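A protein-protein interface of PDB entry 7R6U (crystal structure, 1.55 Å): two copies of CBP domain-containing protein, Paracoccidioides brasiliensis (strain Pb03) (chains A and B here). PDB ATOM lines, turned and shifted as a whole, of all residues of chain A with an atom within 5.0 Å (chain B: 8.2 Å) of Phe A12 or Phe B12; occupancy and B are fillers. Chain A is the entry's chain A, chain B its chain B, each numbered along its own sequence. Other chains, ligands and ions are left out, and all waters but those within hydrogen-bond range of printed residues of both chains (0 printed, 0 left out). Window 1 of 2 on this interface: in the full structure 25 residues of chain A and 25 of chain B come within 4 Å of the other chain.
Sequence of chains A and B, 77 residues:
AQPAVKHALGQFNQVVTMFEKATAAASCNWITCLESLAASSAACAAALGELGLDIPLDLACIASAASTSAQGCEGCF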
ATOM      1  N   ALA A   8     -10.042   3.861  32.774  1.00  0.00           N
ATOM      2  CA  ALA A   8      -9.580   5.224  32.518  1.00  0.00           C
ATOM      3  C   ALA A   8      -8.829   5.314  31.195  1.00  0.00           C
ATOM      4  O   ALA A   8      -8.946   6.308  30.470  1.00  0.00           O
ATOM      5  CB  ALA A   8      -8.694   5.704  33.670  1.00  0.00           C
ATOM      6  N   LEU A   9      -8.039   4.288  30.871  1.00  0.00           N
ATOM      7  CA  LEU A   9      -7.317   4.277  29.602  1.00  0.00           C
ATOM      8  C   LEU A   9      -8.279   4.245  28.420  1.00  0.00           C
ATOM      9  O   LEU A   9      -8.065   4.937  27.417  1.00  0.00           O
ATOM     10  CB  LEU A   9      -6.356   3.081  29.557  1.00  0.00           C
ATOM     11  CG  LEU A   9      -5.115   3.193  30.456  1.00  0.00           C
ATOM     12  CD1 LEU A   9      -4.383   1.859  30.568  1.00  0.00           C
ATOM     13  CD2 LEU A   9      -4.184   4.277  29.936  1.00  0.00           C
ATOM     14  N   GLY A  10      -9.341   3.444  28.517  1.00  0.00           N
ATOM     15  CA  GLY A  10     -10.347   3.440  27.468  1.00  0.00           C
ATOM     16  C   GLY A  10     -11.010   4.793  27.295  1.00  0.00           C
ATOM     17  O   GLY A  10     -11.200   5.264  26.167  1.00  0.00           O
ATOM     18  N   GLN A  11     -11.360   5.446  28.410  1.00  0.00           N
ATOM     19  CA  GLN A  11     -11.961   6.772  28.313  1.00  0.00           C
ATOM     20  C   GLN A  11     -10.985   7.768  27.714  1.00  0.00           C
ATOM     21  O   GLN A  11     -11.381   8.668  26.971  1.00  0.00           O
ATOM     22  CB  GLN A  11     -12.421   7.258  29.683  1.00  0.00           C
ATOM     23  CG  GLN A  11     -13.601   6.508  30.258  1.00  0.00           C
ATOM     24  CD  GLN A  11     -13.846   6.882  31.700  1.00  0.00           C
ATOM     25  OE1 GLN A  11     -12.906   7.156  32.441  1.00  0.00           O
ATOM     26  NE2 GLN A  11     -15.111   6.901  32.107  1.00  0.00           N
ATOM     27  N   PHE A  12      -9.701   7.633  28.041  1.00  0.00           N
ATOM     28  CA  PHE A  12      -8.713   8.545  27.483  1.00  0.00           C
ATOM     29  C   PHE A  12      -8.689   8.472  25.963  1.00  0.00           C
ATOM     30  O   PHE A  12      -8.636   9.504  25.286  1.00  0.00           O
ATOM     31  CB  PHE A  12      -7.331   8.238  28.055  1.00  0.00           C
ATOM     32  CG  PHE A  12      -6.245   9.102  27.491  1.00  0.00           C
ATOM     33  CD1 PHE A  12      -6.218  10.459  27.746  1.00  0.00           C
ATOM     34  CD2 PHE A  12      -5.256   8.551  26.695  1.00  0.00           C
ATOM     35  CE1 PHE A  12      -5.206  11.254  27.231  1.00  0.00           C
ATOM     36  CE2 PHE A  12      -4.248   9.338  26.172  1.00  0.00           C
ATOM     37  CZ  PHE A  12      -4.221  10.682  26.444  1.00  0.00           C
ATOM     38  N   ASN A  13      -8.732   7.264  25.405  1.00  0.00           N
ATOM     39  CA  ASN A  13      -8.720   7.137  23.948  1.00  0.00           C
ATOM     40  C   ASN A  13      -9.909   7.856  23.306  1.00  0.00           C
ATOM     41  O   ASN A  13      -9.765   8.486  22.251  1.00  0.00           O
ATOM     42  CB  ASN A  13      -8.702   5.661  23.555  1.00  0.00           C
ATOM     43  CG  ASN A  13      -7.389   4.970  23.914  1.00  0.00           C
ATOM     44  OD1 ASN A  13      -6.339   5.609  24.010  1.00  0.00           O
ATOM     45  ND2 ASN A  13      -7.445   3.656  24.097  1.00  0.00           N
ATOM     46  N   GLN A  14     -11.081   7.807  23.949  1.00  0.00           N
ATOM     47  CA  GLN A  14     -12.253   8.520  23.435  1.00  0.00           C
ATOM     48  C   GLN A  14     -12.075  10.035  23.532  1.00  0.00           C
ATOM     49  O   GLN A  14     -12.490  10.775  22.625  1.00  0.00           O
ATOM     50  CB  GLN A  14     -13.508   8.056  24.179  1.00  0.00           C
ATOM     51  CG  GLN A  14     -13.887   6.605  23.862  1.00  0.00           C
ATOM     52  CD  GLN A  14     -14.832   5.986  24.873  1.00  0.00           C
ATOM     53  OE1 GLN A  14     -15.225   6.619  25.849  1.00  0.00           O
ATOM     54  NE2 GLN A  14     -15.199   4.731  24.638  1.00  0.00           N
ATOM     55  N   VAL A  15     -11.495  10.518  24.633  1.00  0.00           N
ATOM     56  CA  VAL A  15     -11.256  11.954  24.784  1.00  0.00           C
ATOM     57  C   VAL A  15     -10.293  12.456  23.713  1.00  0.00           C
ATOM     58  O   VAL A  15     -10.511  13.517  23.115  1.00  0.00           O
ATOM     59  CB  VAL A  15     -10.726  12.267  26.199  1.00  0.00           C
ATOM     60  CG1 VAL A  15     -10.256  13.725  26.301  1.00  0.00           C
ATOM     61  CG2 VAL A  15     -11.791  11.982  27.232  1.00  0.00           C
ATOM     62  N   VAL A  16      -9.205  11.715  23.464  1.00  0.00           N
ATOM     63  CA  VAL A  16      -8.237  12.127  22.447  1.00  0.00           C
ATOM     64  C   VAL A  16      -8.903  12.252  21.077  1.00  0.00           C
ATOM     65  O   VAL A  16      -8.687  13.234  20.355  1.00  0.00           O
ATOM     66  CB  VAL A  16      -7.056  11.142  22.404  1.00  0.00           C
ATOM     67  CG1 VAL A  16      -6.209  11.367  21.152  1.00  0.00           C
ATOM     68  CG2 VAL A  16      -6.200  11.310  23.638  1.00  0.00           C
ATOM     69  N   PRO A  56      -2.122  13.166  21.848  1.00  0.00           N
ATOM     70  CA  PRO A  56      -2.051  13.101  23.317  1.00  0.00           C
ATOM     71  C   PRO A  56      -1.104  14.124  23.916  1.00  0.00           C
ATOM     72  O   PRO A  56      -1.416  14.694  24.970  1.00  0.00           O
ATOM     73  CB  PRO A  56      -1.589  11.662  23.583  1.00  0.00           C
ATOM     74  CG  PRO A  56      -2.136  10.900  22.420  1.00  0.00           C
ATOM     75  CD  PRO A  56      -2.006  11.823  21.240  1.00  0.00           C
ATOM     76  N   LEU A  59      -2.759  17.588  23.681  1.00  0.00           N
ATOM     77  CA  LEU A  59      -3.807  17.724  24.679  1.00  0.00           C
ATOM     78  C   LEU A  59      -3.209  18.013  26.048  1.00  0.00           C
ATOM     79  O   LEU A  59      -3.670  18.911  26.765  1.00  0.00           O
ATOM     80  CB  LEU A  59      -4.663  16.454  24.671  1.00  0.00           C
ATOM     81  CG  LEU A  59      -5.768  16.269  25.706  1.00  0.00           C
ATOM     82  CD1 LEU A  59      -6.681  17.480  25.684  1.00  0.00           C
ATOM     83  CD2 LEU A  59      -6.525  14.972  25.426  1.00  0.00           C
ATOM     84  N   ALA A  60      -2.159  17.275  26.427  1.00  0.00           N
ATOM     85  CA  ALA A  60      -1.475  17.554  27.687  1.00  0.00           C
ATOM     86  C   ALA A  60      -0.895  18.965  27.708  1.00  0.00           C
ATOM     87  O   ALA A  60      -0.928  19.647  28.743  1.00  0.00           O
ATOM     88  CB  ALA A  60      -0.369  16.525  27.920  1.00  0.00           C
ATOM     89  N   ALA A  63      -3.860  21.494  28.119  1.00  0.00           N
ATOM     90  CA  ALA A  63      -4.389  21.411  29.475  1.00  0.00           C
ATOM     91  C   ALA A  63      -3.462  22.070  30.483  1.00  0.00           C
ATOM     92  O   ALA A  63      -3.928  22.634  31.480  1.00  0.00           O
ATOM     93  CB  ALA A  63      -4.620  19.950  29.862  1.00  0.00           C
ATOM     94  N   VAL B   5     -14.256  21.861  21.942  1.00  0.00           N
ATOM     95  CA  VAL B   5     -12.884  21.850  22.450  1.00  0.00           C
ATOM     96  C   VAL B   5     -12.888  21.948  23.968  1.00  0.00           C
ATOM     97  O   VAL B   5     -12.207  21.176  24.657  1.00  0.00           O
ATOM     98  CB  VAL B   5     -12.072  23.005  21.837  1.00  0.00           C
ATOM     99  CG1 VAL B   5     -10.647  23.024  22.418  1.00  0.00           C
ATOM    100  CG2 VAL B   5     -11.962  22.874  20.336  1.00  0.00           C
ATOM    101  N   LYS B   6     -13.669  22.889  24.507  1.00  0.00           N
ATOM    102  CA  LYS B   6     -13.725  23.071  25.960  1.00  0.00           C
ATOM    103  C   LYS B   6     -14.285  21.837  26.649  1.00  0.00           C
ATOM    104  O   LYS B   6     -13.760  21.403  27.681  1.00  0.00           O
ATOM    105  CB  LYS B   6     -14.579  24.292  26.309  1.00  0.00           C
ATOM    106  CG  LYS B   6     -13.826  25.605  26.245  1.00  0.00           C
ATOM    107  CD  LYS B   6     -12.854  25.679  27.414  1.00  0.00           C
ATOM    108  CE  LYS B   6     -12.296  27.077  27.603  1.00  0.00           C
ATOM    109  NZ  LYS B   6     -11.751  27.242  28.985  1.00  0.00           N
ATOM    110  N   HIS B   7     -15.315  21.221  26.061  1.00  0.00           N
ATOM    111  CA  HIS B   7     -15.875  20.009  26.651  1.00  0.00           C
ATOM    112  C   HIS B   7     -14.841  18.895  26.727  1.00  0.00           C
ATOM    113  O   HIS B   7     -14.753  18.185  27.737  1.00  0.00           O
ATOM    114  CB  HIS B   7     -17.079  19.541  25.839  1.00  0.00           C
ATOM    115  CG  HIS B   7     -17.757  18.344  26.426  1.00  0.00           C
ATOM    116  ND1 HIS B   7     -17.477  17.057  26.022  1.00  0.00           N
ATOM    117  CD2 HIS B   7     -18.697  18.237  27.391  1.00  0.00           C
ATOM    118  CE1 HIS B   7     -18.215  16.209  26.718  1.00  0.00           C
ATOM    119  NE2 HIS B   7     -18.964  16.899  27.557  1.00  0.00           N
ATOM    120  N   ALA B   8     -14.095  18.685  25.630  1.00  0.00           N
ATOM    121  CA  ALA B   8     -13.074  17.646  25.584  1.00  0.00           C
ATOM    122  C   ALA B   8     -11.975  17.907  26.613  1.00  0.00           C
ATOM    123  O   ALA B   8     -11.515  16.975  27.287  1.00  0.00           O
ATOM    124  CB  ALA B   8     -12.499  17.561  24.171  1.00  0.00           C
ATOM    125  N   LEU B   9     -11.584  19.176  26.790  1.00  0.00           N
ATOM    126  CA  LEU B   9     -10.596  19.497  27.824  1.00  0.00           C
ATOM    127  C   LEU B   9     -11.126  19.171  29.214  1.00  0.00           C
ATOM    128  O   LEU B   9     -10.382  18.667  30.068  1.00  0.00           O
ATOM    129  CB  LEU B   9     -10.178  20.969  27.736  1.00  0.00           C
ATOM    130  CG  LEU B   9      -9.246  21.317  26.564  1.00  0.00           C
ATOM    131  CD1 LEU B   9      -9.157  22.822  26.366  1.00  0.00           C
ATOM    132  CD2 LEU B   9      -7.839  20.717  26.785  1.00  0.00           C
ATOM    133  N   GLY B  10     -12.406  19.463  29.469  1.00  0.00           N
ATOM    134  CA  GLY B  10     -13.004  19.080  30.737  1.00  0.00           C
ATOM    135  C   GLY B  10     -12.980  17.580  30.953  1.00  0.00           C
ATOM    136  O   GLY B  10     -12.649  17.106  32.039  1.00  0.00           O
ATOM    137  N   GLN B  11     -13.301  16.813  29.909  1.00  0.00           N
ATOM    138  CA  GLN B  11     -13.268  15.360  30.042  1.00  0.00           C
ATOM    139  C   GLN B  11     -11.849  14.851  30.275  1.00  0.00           C
ATOM    140  O   GLN B  11     -11.649  13.893  31.033  1.00  0.00           O
ATOM    141  CB  GLN B  11     -13.886  14.718  28.804  1.00  0.00           C
ATOM    142  CG  GLN B  11     -15.389  14.989  28.674  1.00  0.00           C
ATOM    143  CD  GLN B  11     -16.152  14.436  29.856  1.00  0.00           C
ATOM    144  OE1 GLN B  11     -16.127  13.230  30.099  1.00  0.00           O
ATOM    145  NE2 GLN B  11     -16.810  15.313  30.623  1.00  0.00           N
ATOM    146  N   PHE B  12     -10.857  15.478  29.631  1.00  0.00           N
ATOM    147  CA  PHE B  12      -9.458  15.111  29.851  1.00  0.00           C
ATOM    148  C   PHE B  12      -9.065  15.306  31.310  1.00  0.00           C
ATOM    149  O   PHE B  12      -8.442  14.430  31.918  1.00  0.00           O
ATOM    150  CB  PHE B  12      -8.548  15.941  28.947  1.00  0.00           C
ATOM    151  CG  PHE B  12      -7.066  15.692  29.174  1.00  0.00           C
ATOM    152  CD1 PHE B  12      -6.504  14.476  28.852  1.00  0.00           C
ATOM    153  CD2 PHE B  12      -6.262  16.677  29.717  1.00  0.00           C
ATOM    154  CE1 PHE B  12      -5.134  14.247  29.049  1.00  0.00           C
ATOM    155  CE2 PHE B  12      -4.894  16.442  29.926  1.00  0.00           C
ATOM    156  CZ  PHE B  12      -4.354  15.233  29.586  1.00  0.00           C
ATOM    157  N   ASN B  13      -9.422  16.448  31.893  1.00  0.00           N
ATOM    158  CA  ASN B  13      -9.071  16.689  33.291  1.00  0.00           C
ATOM    159  C   ASN B  13      -9.710  15.650  34.205  1.00  0.00           C
ATOM    160  O   ASN B  13      -9.072  15.168  35.150  1.00  0.00           O
ATOM    161  CB  ASN B  13      -9.477  18.103  33.701  1.00  0.00           C
ATOM    162  CG  ASN B  13      -8.625  19.176  33.031  1.00  0.00           C
ATOM    163  OD1 ASN B  13      -7.474  18.940  32.664  1.00  0.00           O
ATOM    164  ND2 ASN B  13      -9.194  20.362  32.874  1.00  0.00           N
ATOM    165  N   GLN B  14     -10.942  15.240  33.896  1.00  0.00           N
ATOM    166  CA  GLN B  14     -11.602  14.214  34.703  1.00  0.00           C
ATOM    167  C   GLN B  14     -10.898  12.870  34.583  1.00  0.00           C
ATOM    168  O   GLN B  14     -10.684  12.182  35.595  1.00  0.00           O
ATOM    169  CB  GLN B  14     -13.059  14.066  34.276  1.00  0.00           C
ATOM    170  CG  GLN B  14     -13.912  15.268  34.619  1.00  0.00           C
ATOM    171  CD  GLN B  14     -14.159  15.375  36.103  1.00  0.00           C
ATOM    172  OE1 GLN B  14     -13.609  16.248  36.776  1.00  0.00           O
ATOM    173  NE2 GLN B  14     -14.994  14.486  36.627  1.00  0.00           N
ATOM    174  N   VAL B  15     -10.512  12.500  33.362  1.00  0.00           N
ATOM    175  CA  VAL B  15      -9.822  11.233  33.132  1.00  0.00           C
ATOM    176  C   VAL B  15      -8.468  11.224  33.831  1.00  0.00           C
ATOM    177  O   VAL B  15      -8.060  10.205  34.398  1.00  0.00           O
ATOM    178  CB  VAL B  15      -9.683  10.951  31.624  1.00  0.00           C
ATOM    179  CG1 VAL B  15      -8.807   9.734  31.376  1.00  0.00           C
ATOM    180  CG2 VAL B  15     -11.053  10.707  31.012  1.00  0.00           C
ATOM    181  N   VAL B  16      -7.742  12.340  33.778  1.00  0.00           N
ATOM    182  CA  VAL B  16      -6.434  12.406  34.434  1.00  0.00           C
ATOM    183  C   VAL B  16      -6.588  12.150  35.927  1.00  0.00           C
ATOM    184  O   VAL B  16      -5.820  11.388  36.529  1.00  0.00           O
ATOM    185  CB  VAL B  16      -5.744  13.759  34.160  1.00  0.00           C
ATOM    186  CG1 VAL B  16      -4.539  13.943  35.107  1.00  0.00           C
ATOM    187  CG2 VAL B  16      -5.270  13.832  32.728  1.00  0.00           C
ATOM    188  N   THR B  17      -7.592  12.782  36.544  1.00  0.00           N
ATOM    189  CA  THR B  17      -7.856  12.573  37.966  1.00  0.00           C
ATOM    190  C   THR B  17      -8.178  11.112  38.257  1.00  0.00           C
ATOM    191  O   THR B  17      -7.646  10.520  39.207  1.00  0.00           O
ATOM    192  CB  THR B  17      -8.994  13.487  38.419  1.00  0.00           C
ATOM    193  OG1 THR B  17      -8.618  14.850  38.184  1.00  0.00           O
ATOM    194  CG2 THR B  17      -9.288  13.276  39.901  1.00  0.00           C
ATOM    195  N   MET B  18      -9.057  10.518  37.450  1.00  0.00           N
ATOM    196  CA  MET B  18      -9.438   9.127  37.660  1.00  0.00           C
ATOM    197  C   MET B  18      -8.243   8.200  37.490  1.00  0.00           C
ATOM    198  O   MET B  18      -8.084   7.236  38.250  1.00  0.00           O
ATOM    199  CB  MET B  18     -10.551   8.741  36.682  1.00  0.00           C
ATOM    200  CG  MET B  18     -11.859   9.461  36.905  1.00  0.00           C
ATOM    201  SD  MET B  18     -13.085   8.988  35.666  1.00  0.00           S
ATOM    202  CE  MET B  18     -12.874   7.205  35.657  1.00  0.00           C
ATOM    203  N   PHE B  19      -7.396   8.482  36.494  1.00  0.00           N
ATOM    204  CA  PHE B  19      -6.210   7.670  36.235  1.00  0.00           C
ATOM    205  C   PHE B  19      -5.208   7.771  37.377  1.00  0.00           C
ATOM    206  O   PHE B  19      -4.625   6.759  37.784  1.00  0.00           O
ATOM    207  CB  PHE B  19      -5.569   8.109  34.918  1.00  0.00           C
ATOM    208  CG  PHE B  19      -4.376   7.290  34.503  1.00  0.00           C
ATOM    209  CD1 PHE B  19      -4.536   5.998  34.030  1.00  0.00           C
ATOM    210  CD2 PHE B  19      -3.112   7.843  34.516  1.00  0.00           C
ATOM    211  CE1 PHE B  19      -3.419   5.259  33.606  1.00  0.00           C
ATOM    212  CE2 PHE B  19      -2.000   7.111  34.107  1.00  0.00           C
ATOM    213  CZ  PHE B  19      -2.158   5.824  33.650  1.00  0.00           C
ATOM    214  N   ASP B  54       4.435  14.073  36.372  1.00  0.00           N
ATOM    215  CA  ASP B  54       3.484  14.742  35.478  1.00  0.00           C
ATOM    216  C   ASP B  54       2.461  13.694  35.041  1.00  0.00           C
ATOM    217  O   ASP B  54       2.722  12.910  34.126  1.00  0.00           O
ATOM    218  CB  ASP B  54       4.265  15.335  34.306  1.00  0.00           C
ATOM    219  CG  ASP B  54       3.442  16.262  33.429  1.00  0.00           C
ATOM    220  OD1 ASP B  54       2.313  15.898  33.050  1.00  0.00           O
ATOM    221  OD2 ASP B  54       3.947  17.363  33.104  1.00  0.00           O
ATOM    222  N   ILE B  55       1.302  13.641  35.722  1.00  0.00           N
ATOM    223  CA  ILE B  55       0.327  12.580  35.434  1.00  0.00           C
ATOM    224  C   ILE B  55      -0.168  12.634  33.995  1.00  0.00           C
ATOM    225  O   ILE B  55      -0.298  11.570  33.368  1.00  0.00           O
ATOM    226  CB  ILE B  55      -0.808  12.602  36.467  1.00  0.00           C
ATOM    227  CG1 ILE B  55      -0.252  12.502  37.888  1.00  0.00           C
ATOM    228  CG2 ILE B  55      -1.764  11.450  36.215  1.00  0.00           C
ATOM    229  CD1 ILE B  55       0.334  11.145  38.209  1.00  0.00           C
ATOM    230  N   PRO B  56      -0.473  13.798  33.402  1.00  0.00           N
ATOM    231  CA  PRO B  56      -0.858  13.780  31.981  1.00  0.00           C
ATOM    232  C   PRO B  56       0.176  13.130  31.075  1.00  0.00           C
ATOM    233  O   PRO B  56      -0.200  12.421  30.140  1.00  0.00           O
ATOM    234  CB  PRO B  56      -1.059  15.266  31.660  1.00  0.00           C
ATOM    235  CG  PRO B  56      -1.496  15.853  32.945  1.00  0.00           C
ATOM    236  CD  PRO B  56      -0.707  15.126  34.007  1.00  0.00           C
ATOM    237  N   LEU B  57       1.475  13.342  31.320  1.00  0.00           N
ATOM    238  CA  LEU B  57       2.478  12.673  30.493  1.00  0.00           C
ATOM    239  C   LEU B  57       2.545  11.182  30.794  1.00  0.00           C
ATOM    240  O   LEU B  57       2.757  10.379  29.879  1.00  0.00           O
ATOM    241  CB  LEU B  57       3.854  13.313  30.692  1.00  0.00           C
ATOM    242  CG  LEU B  57       4.030  14.718  30.106  1.00  0.00           C
ATOM    243  CD1 LEU B  57       5.426  15.231  30.456  1.00  0.00           C
ATOM    244  CD2 LEU B  57       3.820  14.702  28.589  1.00  0.00           C
ATOM    245  N   ASP B  58       2.394  10.798  32.071  1.00  0.00           N
ATOM    246  CA  ASP B  58       2.330   9.379  32.424  1.00  0.00           C
ATOM    247  C   ASP B  58       1.193   8.695  31.684  1.00  0.00           C
ATOM    248  O   ASP B  58       1.348   7.584  31.165  1.00  0.00           O
ATOM    249  CB  ASP B  58       2.112   9.181  33.925  1.00  0.00           C
ATOM    250  CG  ASP B  58       3.242   9.709  34.785  1.00  0.00           C
ATOM    251  OD1 ASP B  58       4.381   9.934  34.306  1.00  0.00           O
ATOM    252  OD2 ASP B  58       2.971   9.882  35.990  1.00  0.00           O
ATOM    253  N   LEU B  59       0.035   9.351  31.640  1.00  0.00           N
ATOM    254  CA  LEU B  59      -1.134   8.792  30.971  1.00  0.00           C
ATOM    255  C   LEU B  59      -0.888   8.641  29.473  1.00  0.00           C
ATOM    256  O   LEU B  59      -1.134   7.577  28.899  1.00  0.00           O
ATOM    257  CB  LEU B  59      -2.339   9.687  31.255  1.00  0.00           C
ATOM    258  CG  LEU B  59      -3.631   9.346  30.516  1.00  0.00           C
ATOM    259  CD1 LEU B  59      -4.051   7.894  30.708  1.00  0.00           C
ATOM    260  CD2 LEU B  59      -4.703  10.300  30.991  1.00  0.00           C
ATOM    261  N   ALA B  60      -0.354   9.682  28.830  1.00  0.00           N
ATOM    262  CA  ALA B  60      -0.036   9.580  27.406  1.00  0.00           C
ATOM    263  C   ALA B  60       0.977   8.472  27.139  1.00  0.00           C
ATOM    264  O   ALA B  60       0.884   7.760  26.128  1.00  0.00           O
ATOM    265  CB  ALA B  60       0.483  10.917  26.887  1.00  0.00           C
ATOM    266  N   CYS B  61       1.956   8.314  28.028  1.00  0.00           N
ATOM    267  CA  CYS B  61       2.920   7.229  27.870  1.00  0.00           C
ATOM    268  C   CYS B  61       2.233   5.864  27.908  1.00  0.00           C
ATOM    269  O   CYS B  61       2.448   5.025  27.023  1.00  0.00           O
ATOM    270  CB  CYS B  61       4.008   7.322  28.945  1.00  0.00           C
ATOM    271  SG  CYS B  61       5.050   5.856  29.032  1.00  0.00           S
ATOM    272  N   ILE B  62       1.428   5.606  28.947  1.00  0.00           N
ATOM    273  CA  ILE B  62       0.795   4.295  29.083  1.00  0.00           C
ATOM    274  C   ILE B  62      -0.152   4.023  27.910  1.00  0.00           C
ATOM    275  O   ILE B  62      -0.222   2.899  27.398  1.00  0.00           O
ATOM    276  CB  ILE B  62       0.084   4.179  30.447  1.00  0.00           C
ATOM    277  CG1 ILE B  62       1.121   4.146  31.582  1.00  0.00           C
ATOM    278  CG2 ILE B  62      -0.755   2.910  30.504  1.00  0.00           C
ATOM    279  CD1 ILE B  62       2.117   3.014  31.456  1.00  0.00           C
ATOM    280  N   ALA B  63      -0.889   5.047  27.466  1.00  0.00           N
ATOM    281  CA  ALA B  63      -1.783   4.861  26.326  1.00  0.00           C
ATOM    282  C   ALA B  63      -1.007   4.505  25.061  1.00  0.00           C
ATOM    283  O   ALA B  63      -1.508   3.752  24.220  1.00  0.00           O
ATOM    284  CB  ALA B  63      -2.620   6.120  26.110  1.00  0.00           C
ATOM    285  N   SER B  64       0.226   5.005  24.923  1.00  0.00           N
ATOM    286  CA  SER B  64       1.030   4.739  23.734  1.00  0.00           C
ATOM    287  C   SER B  64       1.678   3.366  23.757  1.00  0.00           C
ATOM    288  O   SER B  64       2.112   2.884  22.702  1.00  0.00           O
ATOM    289  CB  SER B  64       2.119   5.809  23.576  1.00  0.00           C
ATOM    290  OG  SER B  64       3.228   5.579  24.452  1.00  0.00           O
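The side-chain amide oxygen (OE1) of Gln A11 sits close to the side-chain sulfur (SD) of Met B18 (3.7 Å).
ND2 of Asn B13 sits close to O of Leu B9 (3.5 Å).
Among the printed residues, merely in contact across the chains: Ala A8 with Val B15 (3.5 Å), Leu A9 with Phe B19 (3.9 Å), Leu A9 with Leu B59 (3.7 Å), Leu A9 with Ile B62 (3.7 Å), Gln A11 with Val B15 (3.9 Å), Phe A12 with Phe B12 (3.5 Å), Phe A12 with Val B15 (3.9 Å), Phe A12 with Leu B59 (3.6 Å), Phe A12 with Ala B63 (3.6 Å), Val A15 with Ala B8 (3.6 Å), Val A15 with Gln B11 (3.8 Å), Val A15 with Phe B12 (3.8 Å), Pro A56 with Ala B60 (3.97 Å), Leu A59 with Leu B9 (3.6 Å), Leu A59 with Phe B12 (3.5 Å) and Ala A63 with Phe B12 (3.5 Å).
Of chain B, only Phe B12 (3.5 Å), Val B15 (3.9 Å), Leu B59 (3.6 Å) and Ala B63 (3.6 Å) come within 4 Å of Phe A12. Printed residues of chain B within 4 Å of Leu A59: Leu B9 and Phe B12. Printed residues of chain B within 4 Å of Ala A63: Phe B12. His B7 touches none of the printed residues of chain A. Phe B12 touches four residues of chain A. Of the printed residues of chain A, Val B15 touches Ala A8, Gln A11 and Phe A12. The nearest residue of chain B that does not touch Phe A12 is Ala B60 (4.4 Å). The nearest residue of chain A that does not touch Phe B12 is Ala A60 (4.2 Å). The nearest printed residue of chain B that does not touch Gln A11 is Gln B14 (6.3 Å).
Printed residues of chain A that touch a printed residue of chain B: Ala A8, Leu A9, Gln A11, Phe A12, Val A15, Pro A56, Leu A59 and Ala A63. Hydrophobic or aromatic side chains of chain A that line the printed part of chain B: Leu A9, Phe A12, Val A15, Pro A56, Leu A59 and Ala A63. Of the 26 printed residues of chain B, 11 touch a printed residue of chain A. Hydrophobic or aromatic side chains of chain B that line the printed part of chain A: Leu B9, Phe B12, Val B15, Met B18, Phe B19, Leu B59, Ala B60, Ile B62 and Ala B63. Among the printed residues, 17 pairs touch across the chains. Among the printed residues, no Asp or Glu carboxylate lies within 4 Å of a Lys or Arg side-chain nitrogen of the other chain.
Leu A9 touches Leu B59, and with the chains exchanged Leu A59 touches Leu B9. Phe A12 touches its own counterpart, Phe B12. Phe A12 touches Leu B59, and with the chains exchanged Leu A59 touches Phe B12. Phe A12 touches Ala B63, and with the chains exchanged Ala A63 touches Phe B12. 13 positions are printed for both chains.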
